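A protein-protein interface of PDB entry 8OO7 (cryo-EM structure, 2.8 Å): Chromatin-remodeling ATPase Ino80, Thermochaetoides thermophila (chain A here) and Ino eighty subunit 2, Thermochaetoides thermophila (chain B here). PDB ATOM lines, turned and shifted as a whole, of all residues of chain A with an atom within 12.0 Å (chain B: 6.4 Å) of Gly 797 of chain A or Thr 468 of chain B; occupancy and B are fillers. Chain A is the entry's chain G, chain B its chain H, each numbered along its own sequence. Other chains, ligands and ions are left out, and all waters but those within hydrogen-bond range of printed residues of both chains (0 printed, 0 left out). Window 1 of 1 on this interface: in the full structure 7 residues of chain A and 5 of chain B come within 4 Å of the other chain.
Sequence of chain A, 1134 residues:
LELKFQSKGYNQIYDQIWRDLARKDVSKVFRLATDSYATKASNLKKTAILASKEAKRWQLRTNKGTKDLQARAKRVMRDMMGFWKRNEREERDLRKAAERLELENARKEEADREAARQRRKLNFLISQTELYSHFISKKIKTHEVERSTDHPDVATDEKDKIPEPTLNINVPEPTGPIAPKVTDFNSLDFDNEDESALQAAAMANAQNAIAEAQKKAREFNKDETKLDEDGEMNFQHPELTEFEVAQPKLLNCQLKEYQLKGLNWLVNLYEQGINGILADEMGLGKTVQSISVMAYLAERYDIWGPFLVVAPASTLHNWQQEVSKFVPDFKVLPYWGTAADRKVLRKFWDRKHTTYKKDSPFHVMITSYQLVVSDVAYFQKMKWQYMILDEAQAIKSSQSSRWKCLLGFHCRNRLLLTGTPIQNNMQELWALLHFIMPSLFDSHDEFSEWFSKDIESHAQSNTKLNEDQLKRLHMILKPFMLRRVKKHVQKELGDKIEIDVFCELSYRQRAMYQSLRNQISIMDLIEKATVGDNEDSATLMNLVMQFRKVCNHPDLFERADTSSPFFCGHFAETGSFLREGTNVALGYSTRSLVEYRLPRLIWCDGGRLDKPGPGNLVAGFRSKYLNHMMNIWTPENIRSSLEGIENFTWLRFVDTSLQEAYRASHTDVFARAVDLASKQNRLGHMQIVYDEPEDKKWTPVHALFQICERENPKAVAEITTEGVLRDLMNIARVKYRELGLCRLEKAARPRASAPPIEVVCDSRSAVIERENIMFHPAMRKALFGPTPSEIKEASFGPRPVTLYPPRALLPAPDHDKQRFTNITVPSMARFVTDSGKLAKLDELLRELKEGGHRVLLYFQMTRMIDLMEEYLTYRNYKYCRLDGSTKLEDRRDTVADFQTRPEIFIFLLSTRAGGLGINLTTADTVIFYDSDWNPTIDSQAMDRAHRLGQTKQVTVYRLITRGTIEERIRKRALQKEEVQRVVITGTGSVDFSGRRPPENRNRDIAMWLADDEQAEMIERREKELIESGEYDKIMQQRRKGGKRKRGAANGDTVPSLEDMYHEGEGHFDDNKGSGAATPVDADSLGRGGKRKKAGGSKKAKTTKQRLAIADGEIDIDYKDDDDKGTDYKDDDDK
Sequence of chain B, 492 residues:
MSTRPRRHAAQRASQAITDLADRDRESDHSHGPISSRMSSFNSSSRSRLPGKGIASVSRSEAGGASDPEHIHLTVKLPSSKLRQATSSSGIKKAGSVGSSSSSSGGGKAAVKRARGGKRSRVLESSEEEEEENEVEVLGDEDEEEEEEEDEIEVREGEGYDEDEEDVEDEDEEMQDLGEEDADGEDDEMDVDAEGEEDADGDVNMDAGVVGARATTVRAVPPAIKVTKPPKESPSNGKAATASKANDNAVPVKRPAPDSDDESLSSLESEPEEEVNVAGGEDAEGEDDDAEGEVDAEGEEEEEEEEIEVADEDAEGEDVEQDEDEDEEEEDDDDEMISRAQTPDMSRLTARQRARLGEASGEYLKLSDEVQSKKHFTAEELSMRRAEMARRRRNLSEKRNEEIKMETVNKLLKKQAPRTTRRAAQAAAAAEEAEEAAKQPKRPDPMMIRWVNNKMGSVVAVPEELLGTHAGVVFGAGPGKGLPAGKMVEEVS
NE2 of His 469 of chain B is in hydrogen-bond range of O of Ala 794 of chain A (2.7 Å). The backbone NH of His 469 of chain B is in hydrogen-bond range of the backbone carbonyl oxygen of Gly 797 of chain A. The backbone NH (N) of His 469 of chain B lies close to the backbone carbonyl oxygen (O) of Pro 798 of chain A (3.4 Å).
The backbone carbonyl oxygen (O) of Ile 791 of chain A sits at hydrogen-bond distance from the side-chain hydroxyl (OG) of Ser 795 of chain A (2.8 Å). The backbone carbonyl oxygen (O) of Lys 792 of chain A is in hydrogen-bond range of the side-chain hydroxyl (OG) of Ser 795 of chain A (3.0 Å). OG1 of Thr 468 of chain B sits at hydrogen-bond distance from O of Leu 465 of chain B, 2.5 Å away. N of Ala 470 of chain B lies close to OG1 of Thr 468 of chain B.
Among the printed residues, merely in contact across the chains: Pro 798 of chain A with Pro 478 of chain B, Gly 797 of chain A with Thr 468 of chain B, Pro 800 of chain A with His 469 of chain B, Phe 796 of chain A with Thr 468 of chain B, Arg 799 of chain A with His 469 of chain B, Phe 796 of chain A with Leu 465 of chain B and Ser 795 of chain A with Thr 468 of chain B.
Gly 797 of chain A touches just these residues of chain B: Thr 468 (3.5 Å) and His 469 (3.1 Å). Of the printed residues of chain A, Thr 468 of chain B touches Ser 795 (3.9 Å), Phe 796 (3.6 Å) and Gly 797 (3.5 Å). Leu 465 of chain B touches one residue of chain A. No residue of chain A comes within 4 Å of Gly 467 of chain B. Ala 470 of chain B touches none of the printed residues of chain A. No residue of chain A comes within 4 Å of Gly 471 of chain B. Ala 476 of chain B touches none of the printed residues of chain A. No residue of chain A comes within 4 Å of Gly 477 of chain B. Printed residues of chain A within 4 Å of Pro 478 of chain B: Pro 798 (3.3 Å). Printed residues of chain B within 4 Å of Pro 800 of chain A: His 469. Printed residues of chain B within 4 Å of Ala 794 of chain A: His 469. Leu 803 of chain A touches none of the printed residues of chain B. Lys 792 of chain A touches none of the printed residues of chain B.
Among the printed residues, 10 pairs touch across the chains.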
ATOM      1  N   PRO A 788     -24.929   2.696  25.262  1.00  0.00           N
ATOM      2  CA  PRO A 788     -24.763   4.159  25.142  1.00  0.00           C
ATOM      3  C   PRO A 788     -24.111   4.848  26.333  1.00  0.00           C
ATOM      4  O   PRO A 788     -23.321   5.779  26.136  1.00  0.00           O
ATOM      5  CB  PRO A 788     -26.201   4.649  24.911  1.00  0.00           C
ATOM      6  CG  PRO A 788     -26.837   3.525  24.204  1.00  0.00           C
ATOM      7  CD  PRO A 788     -26.289   2.294  24.862  1.00  0.00           C
ATOM      8  N   SER A 789     -24.429   4.439  27.564  1.00  0.00           N
ATOM      9  CA  SER A 789     -23.721   4.979  28.723  1.00  0.00           C
ATOM     10  C   SER A 789     -22.237   4.631  28.706  1.00  0.00           C
ATOM     11  O   SER A 789     -21.403   5.434  29.138  1.00  0.00           O
ATOM     12  CB  SER A 789     -24.361   4.479  30.015  1.00  0.00           C
ATOM     13  OG  SER A 789     -23.707   5.024  31.147  1.00  0.00           O
ATOM     14  N   GLU A 790     -21.884   3.444  28.213  1.00  0.00           N
ATOM     15  CA  GLU A 790     -20.469   3.100  28.089  1.00  0.00           C
ATOM     16  C   GLU A 790     -19.756   4.007  27.091  1.00  0.00           C
ATOM     17  O   GLU A 790     -18.596   4.378  27.301  1.00  0.00           O
ATOM     18  CB  GLU A 790     -20.312   1.634  27.684  1.00  0.00           C
ATOM     19  CG  GLU A 790     -21.026   0.653  28.594  1.00  0.00           C
ATOM     20  CD  GLU A 790     -20.888  -0.778  28.119  1.00  0.00           C
ATOM     21  OE1 GLU A 790     -21.022  -1.018  26.901  1.00  0.00           O
ATOM     22  OE2 GLU A 790     -20.637  -1.664  28.964  1.00  0.00           O
ATOM     23  N   ILE A 791     -20.428   4.364  25.996  1.00  0.00           N
ATOM     24  CA  ILE A 791     -19.855   5.299  25.031  1.00  0.00           C
ATOM     25  C   ILE A 791     -19.674   6.682  25.647  1.00  0.00           C
ATOM     26  O   ILE A 791     -18.665   7.357  25.408  1.00  0.00           O
ATOM     27  CB  ILE A 791     -20.738   5.354  23.772  1.00  0.00           C
ATOM     28  CG1 ILE A 791     -20.806   3.978  23.110  1.00  0.00           C
ATOM     29  CG2 ILE A 791     -20.212   6.393  22.793  1.00  0.00           C
ATOM     30  CD1 ILE A 791     -21.840   3.883  22.012  1.00  0.00           C
ATOM     31  N   LYS A 792     -20.644   7.127  26.446  1.00  0.00           N
ATOM     32  CA  LYS A 792     -20.515   8.398  27.157  1.00  0.00           C
ATOM     33  C   LYS A 792     -19.354   8.381  28.144  1.00  0.00           C
ATOM     34  O   LYS A 792     -18.509   9.284  28.139  1.00  0.00           O
ATOM     35  CB  LYS A 792     -21.832   8.729  27.859  1.00  0.00           C
ATOM     36  CG  LYS A 792     -22.961   9.028  26.888  1.00  0.00           C
ATOM     37  CD  LYS A 792     -24.318   9.051  27.569  1.00  0.00           C
ATOM     38  CE  LYS A 792     -25.433   9.155  26.541  1.00  0.00           C
ATOM     39  NZ  LYS A 792     -26.781   9.150  27.169  1.00  0.00           N
ATOM     40  N   GLU A 793     -19.294   7.360  29.001  1.00  0.00           N
ATOM     41  CA  GLU A 793     -18.191   7.237  29.952  1.00  0.00           C
ATOM     42  C   GLU A 793     -16.838   7.216  29.248  1.00  0.00           C
ATOM     43  O   GLU A 793     -15.895   7.899  29.664  1.00  0.00           O
ATOM     44  CB  GLU A 793     -18.364   5.976  30.798  1.00  0.00           C
ATOM     45  CG  GLU A 793     -19.440   6.077  31.864  1.00  0.00           C
ATOM     46  CD  GLU A 793     -19.586   4.798  32.666  1.00  0.00           C
ATOM     47  OE1 GLU A 793     -18.837   3.837  32.395  1.00  0.00           O
ATOM     48  OE2 GLU A 793     -20.451   4.754  33.566  1.00  0.00           O
ATOM     49  N   ALA A 794     -16.725   6.434  28.176  1.00  0.00           N
ATOM     50  CA  ALA A 794     -15.468   6.347  27.437  1.00  0.00           C
ATOM     51  C   ALA A 794     -15.090   7.664  26.766  1.00  0.00           C
ATOM     52  O   ALA A 794     -13.903   8.002  26.691  1.00  0.00           O
ATOM     53  CB  ALA A 794     -15.556   5.232  26.397  1.00  0.00           C
ATOM     54  N   SER A 795     -16.068   8.425  26.275  1.00  0.00           N
ATOM     55  CA  SER A 795     -15.736   9.673  25.592  1.00  0.00           C
ATOM     56  C   SER A 795     -15.499  10.850  26.532  1.00  0.00           C
ATOM     57  O   SER A 795     -14.761  11.774  26.172  1.00  0.00           O
ATOM     58  CB  SER A 795     -16.844  10.031  24.598  1.00  0.00           C
ATOM     59  OG  SER A 795     -18.104  10.106  25.244  1.00  0.00           O
ATOM     60  N   PHE A 796     -16.091  10.853  27.725  1.00  0.00           N
ATOM     61  CA  PHE A 796     -15.872  11.932  28.682  1.00  0.00           C
ATOM     62  C   PHE A 796     -14.804  11.632  29.726  1.00  0.00           C
ATOM     63  O   PHE A 796     -14.524  12.496  30.563  1.00  0.00           O
ATOM     64  CB  PHE A 796     -17.185  12.301  29.379  1.00  0.00           C
ATOM     65  CG  PHE A 796     -18.242  12.809  28.441  1.00  0.00           C
ATOM     66  CD1 PHE A 796     -17.992  13.907  27.634  1.00  0.00           C
ATOM     67  CD2 PHE A 796     -19.483  12.202  28.374  1.00  0.00           C
ATOM     68  CE1 PHE A 796     -18.957  14.384  26.771  1.00  0.00           C
ATOM     69  CE2 PHE A 796     -20.454  12.676  27.512  1.00  0.00           C
ATOM     70  CZ  PHE A 796     -20.190  13.768  26.709  1.00  0.00           C
ATOM     71  N   GLY A 797     -14.208  10.444  29.712  1.00  0.00           N
ATOM     72  CA  GLY A 797     -13.237  10.076  30.715  1.00  0.00           C
ATOM     73  C   GLY A 797     -11.987  10.932  30.665  1.00  0.00           C
ATOM     74  O   GLY A 797     -11.671  11.554  29.646  1.00  0.00           O
ATOM     75  N   PRO A 798     -11.248  10.985  31.777  1.00  0.00           N
ATOM     76  CA  PRO A 798      -9.991  11.746  31.777  1.00  0.00           C
ATOM     77  C   PRO A 798      -8.884  11.065  30.995  1.00  0.00           C
ATOM     78  O   PRO A 798      -8.049  11.752  30.395  1.00  0.00           O
ATOM     79  CB  PRO A 798      -9.647  11.852  33.268  1.00  0.00           C
ATOM     80  CG  PRO A 798     -10.233  10.617  33.859  1.00  0.00           C
ATOM     81  CD  PRO A 798     -11.511  10.361  33.085  1.00  0.00           C
ATOM     82  N   ARG A 799      -8.851   9.738  30.990  1.00  0.00           N
ATOM     83  CA  ARG A 799      -7.883   8.954  30.245  1.00  0.00           C
ATOM     84  C   ARG A 799      -8.613   7.960  29.356  1.00  0.00           C
ATOM     85  O   ARG A 799      -9.712   7.513  29.697  1.00  0.00           O
ATOM     86  CB  ARG A 799      -6.925   8.207  31.184  1.00  0.00           C
ATOM     87  CG  ARG A 799      -5.867   9.100  31.803  1.00  0.00           C
ATOM     88  CD  ARG A 799      -5.110   8.400  32.920  1.00  0.00           C
ATOM     89  NE  ARG A 799      -3.941   9.165  33.339  1.00  0.00           N
ATOM     90  CZ  ARG A 799      -3.988  10.288  34.044  1.00  0.00           C
ATOM     91  NH1 ARG A 799      -5.140  10.830  34.406  1.00  0.00           N
ATOM     92  NH2 ARG A 799      -2.852  10.891  34.379  1.00  0.00           N
ATOM     93  N   PRO A 800      -8.037   7.615  28.204  1.00  0.00           N
ATOM     94  CA  PRO A 800      -8.705   6.673  27.303  1.00  0.00           C
ATOM     95  C   PRO A 800      -8.990   5.346  27.987  1.00  0.00           C
ATOM     96  O   PRO A 800      -8.262   4.910  28.882  1.00  0.00           O
ATOM     97  CB  PRO A 800      -7.703   6.507  26.152  1.00  0.00           C
ATOM     98  CG  PRO A 800      -6.861   7.737  26.205  1.00  0.00           C
ATOM     99  CD  PRO A 800      -6.742   8.058  27.666  1.00  0.00           C
ATOM    100  N   VAL A 801     -10.074   4.710  27.557  1.00  0.00           N
ATOM    101  CA  VAL A 801     -10.458   3.385  28.027  1.00  0.00           C
ATOM    102  C   VAL A 801     -10.900   2.565  26.824  1.00  0.00           C
ATOM    103  O   VAL A 801     -11.614   3.062  25.946  1.00  0.00           O
ATOM    104  CB  VAL A 801     -11.560   3.454  29.109  1.00  0.00           C
ATOM    105  CG1 VAL A 801     -12.834   4.067  28.559  1.00  0.00           C
ATOM    106  CG2 VAL A 801     -11.834   2.071  29.680  1.00  0.00           C
ATOM    107  N   THR A 802     -10.444   1.319  26.767  1.00  0.00           N
ATOM    108  CA  THR A 802     -10.863   0.406  25.714  1.00  0.00           C
ATOM    109  C   THR A 802     -12.200  -0.220  26.085  1.00  0.00           C
ATOM    110  O   THR A 802     -12.320  -0.883  27.119  1.00  0.00           O
ATOM    111  CB  THR A 802      -9.807  -0.673  25.495  1.00  0.00           C
ATOM    112  OG1 THR A 802      -9.506  -1.306  26.744  1.00  0.00           O
ATOM    113  CG2 THR A 802      -8.537  -0.058  24.936  1.00  0.00           C
ATOM    114  N   LEU A 803     -13.200  -0.008  25.234  1.00  0.00           N
ATOM    115  CA  LEU A 803     -14.502  -0.621  25.414  1.00  0.00           C
ATOM    116  C   LEU A 803     -14.456  -2.101  25.052  1.00  0.00           C
ATOM    117  O   LEU A 803     -13.510  -2.594  24.431  1.00  0.00           O
ATOM    118  CB  LEU A 803     -15.558   0.092  24.569  1.00  0.00           C
ATOM    119  CG  LEU A 803     -15.961   1.494  25.025  1.00  0.00           C
ATOM    120  CD1 LEU A 803     -16.821   2.160  23.965  1.00  0.00           C
ATOM    121  CD2 LEU A 803     -16.686   1.440  26.360  1.00  0.00           C
ATOM    122  N   GLU B 464     -17.179  20.579  26.108  1.00  0.00           N
ATOM    123  CA  GLU B 464     -17.291  19.415  26.982  1.00  0.00           C
ATOM    124  C   GLU B 464     -16.153  18.414  26.818  1.00  0.00           C
ATOM    125  O   GLU B 464     -15.888  17.649  27.751  1.00  0.00           O
ATOM    126  CB  GLU B 464     -18.622  18.694  26.746  1.00  0.00           C
ATOM    127  CG  GLU B 464     -19.856  19.465  27.175  1.00  0.00           C
ATOM    128  CD  GLU B 464     -20.194  20.608  26.244  1.00  0.00           C
ATOM    129  OE1 GLU B 464     -19.675  20.630  25.110  1.00  0.00           O
ATOM    130  OE2 GLU B 464     -20.982  21.482  26.651  1.00  0.00           O
ATOM    131  N   LEU B 465     -15.482  18.388  25.669  1.00  0.00           N
ATOM    132  CA  LEU B 465     -14.387  17.449  25.468  1.00  0.00           C
ATOM    133  C   LEU B 465     -13.030  18.003  25.875  1.00  0.00           C
ATOM    134  O   LEU B 465     -12.118  17.219  26.155  1.00  0.00           O
ATOM    135  CB  LEU B 465     -14.341  17.000  24.006  1.00  0.00           C
ATOM    136  CG  LEU B 465     -15.602  16.276  23.530  1.00  0.00           C
ATOM    137  CD1 LEU B 465     -15.356  15.597  22.202  1.00  0.00           C
ATOM    138  CD2 LEU B 465     -16.075  15.267  24.567  1.00  0.00           C
ATOM    139  N   LEU B 466     -12.872  19.322  25.912  1.00  0.00           N
ATOM    140  CA  LEU B 466     -11.696  19.911  26.538  1.00  0.00           C
ATOM    141  C   LEU B 466     -11.644  19.521  28.010  1.00  0.00           C
ATOM    142  O   LEU B 466     -12.639  19.633  28.731  1.00  0.00           O
ATOM    143  CB  LEU B 466     -11.710  21.430  26.380  1.00  0.00           C
ATOM    144  CG  LEU B 466     -11.989  21.935  24.966  1.00  0.00           C
ATOM    145  CD1 LEU B 466     -11.847  23.444  24.902  1.00  0.00           C
ATOM    146  CD2 LEU B 466     -11.059  21.267  23.968  1.00  0.00           C
ATOM    147  N   GLY B 467     -10.478  19.056  28.453  1.00  0.00           N
ATOM    148  CA  GLY B 467     -10.335  18.462  29.765  1.00  0.00           C
ATOM    149  C   GLY B 467     -10.645  16.983  29.835  1.00  0.00           C
ATOM    150  O   GLY B 467     -10.473  16.383  30.903  1.00  0.00           O
ATOM    151  N   THR B 468     -11.102  16.379  28.743  1.00  0.00           N
ATOM    152  CA  THR B 468     -11.144  14.932  28.593  1.00  0.00           C
ATOM    153  C   THR B 468      -9.893  14.458  27.858  1.00  0.00           C
ATOM    154  O   THR B 468      -9.099  15.255  27.353  1.00  0.00           O
ATOM    155  CB  THR B 468     -12.409  14.492  27.850  1.00  0.00           C
ATOM    156  OG1 THR B 468     -12.261  14.760  26.450  1.00  0.00           O
ATOM    157  CG2 THR B 468     -13.619  15.240  28.380  1.00  0.00           C
ATOM    158  N   HIS B 469      -9.718  13.135  27.810  1.00  0.00           N
ATOM    159  CA  HIS B 469      -8.620  12.569  27.030  1.00  0.00           C
ATOM    160  C   HIS B 469      -8.695  12.962  25.559  1.00  0.00           C
ATOM    161  O   HIS B 469      -7.658  13.086  24.899  1.00  0.00           O
ATOM    162  CB  HIS B 469      -8.603  11.049  27.185  1.00  0.00           C
ATOM    163  CG  HIS B 469      -9.769  10.357  26.547  1.00  0.00           C
ATOM    164  ND1 HIS B 469      -9.875  10.170  25.185  1.00  0.00           N
ATOM    165  CD2 HIS B 469     -10.872   9.791  27.092  1.00  0.00           C
ATOM    166  CE1 HIS B 469     -10.999   9.529  24.919  1.00  0.00           C
ATOM    167  NE2 HIS B 469     -11.621   9.286  26.057  1.00  0.00           N
ATOM    168  N   ALA B 470      -9.902  13.152  25.025  1.00  0.00           N
ATOM    169  CA  ALA B 470     -10.054  13.555  23.631  1.00  0.00           C
ATOM    170  C   ALA B 470      -9.543  14.967  23.365  1.00  0.00           C
ATOM    171  O   ALA B 470      -9.331  15.325  22.202  1.00  0.00           O
ATOM    172  CB  ALA B 470     -11.520  13.447  23.212  1.00  0.00           C
ATOM    173  N   GLY B 471      -9.351  15.774  24.412  1.00  0.00           N
ATOM    174  CA  GLY B 471      -8.706  17.071  24.281  1.00  0.00           C
ATOM    175  C   GLY B 471      -7.194  17.041  24.204  1.00  0.00           C
ATOM    176  O   GLY B 471      -6.591  18.033  23.781  1.00  0.00           O
ATOM    177  N   VAL B 472      -6.571  15.931  24.609  1.00  0.00           N
ATOM    178  CA  VAL B 472      -5.113  15.870  24.717  1.00  0.00           C
ATOM    179  C   VAL B 472      -4.451  16.138  23.369  1.00  0.00           C
ATOM    180  O   VAL B 472      -3.415  16.809  23.294  1.00  0.00           O
ATOM    181  CB  VAL B 472      -4.682  14.507  25.296  1.00  0.00           C
ATOM    182  CG1 VAL B 472      -3.172  14.356  25.250  1.00  0.00           C
ATOM    183  CG2 VAL B 472      -5.185  14.343  26.720  1.00  0.00           C
ATOM    184  N   ALA B 476      -5.429  20.292  25.104  1.00  0.00           N
ATOM    185  CA  ALA B 476      -6.485  20.669  26.036  1.00  0.00           C
ATOM    186  C   ALA B 476      -6.966  19.444  26.796  1.00  0.00           C
ATOM    187  O   ALA B 476      -8.166  19.256  27.017  1.00  0.00           O
ATOM    188  CB  ALA B 476      -7.647  21.348  25.314  1.00  0.00           C
ATOM    189  N   GLY B 477      -6.031  18.598  27.217  1.00  0.00           N
ATOM    190  CA  GLY B 477      -6.345  17.473  28.063  1.00  0.00           C
ATOM    191  C   GLY B 477      -6.756  17.881  29.460  1.00  0.00           C
ATOM    192  O   GLY B 477      -6.978  19.061  29.750  1.00  0.00           O
ATOM    193  N   PRO B 478      -6.878  16.895  30.362  1.00  0.00           N
ATOM    194  CA  PRO B 478      -7.199  17.102  31.777  1.00  0.00           C
ATOM    195  C   PRO B 478      -6.304  18.142  32.450  1.00  0.00           C
ATOM    196  O   PRO B 478      -5.157  18.304  32.035  1.00  0.00           O
ATOM    197  CB  PRO B 478      -6.979  15.716  32.397  1.00  0.00           C
ATOM    198  CG  PRO B 478      -7.174  14.767  31.275  1.00  0.00           C
ATOM    199  CD  PRO B 478      -6.663  15.473  30.051  1.00  0.00           C
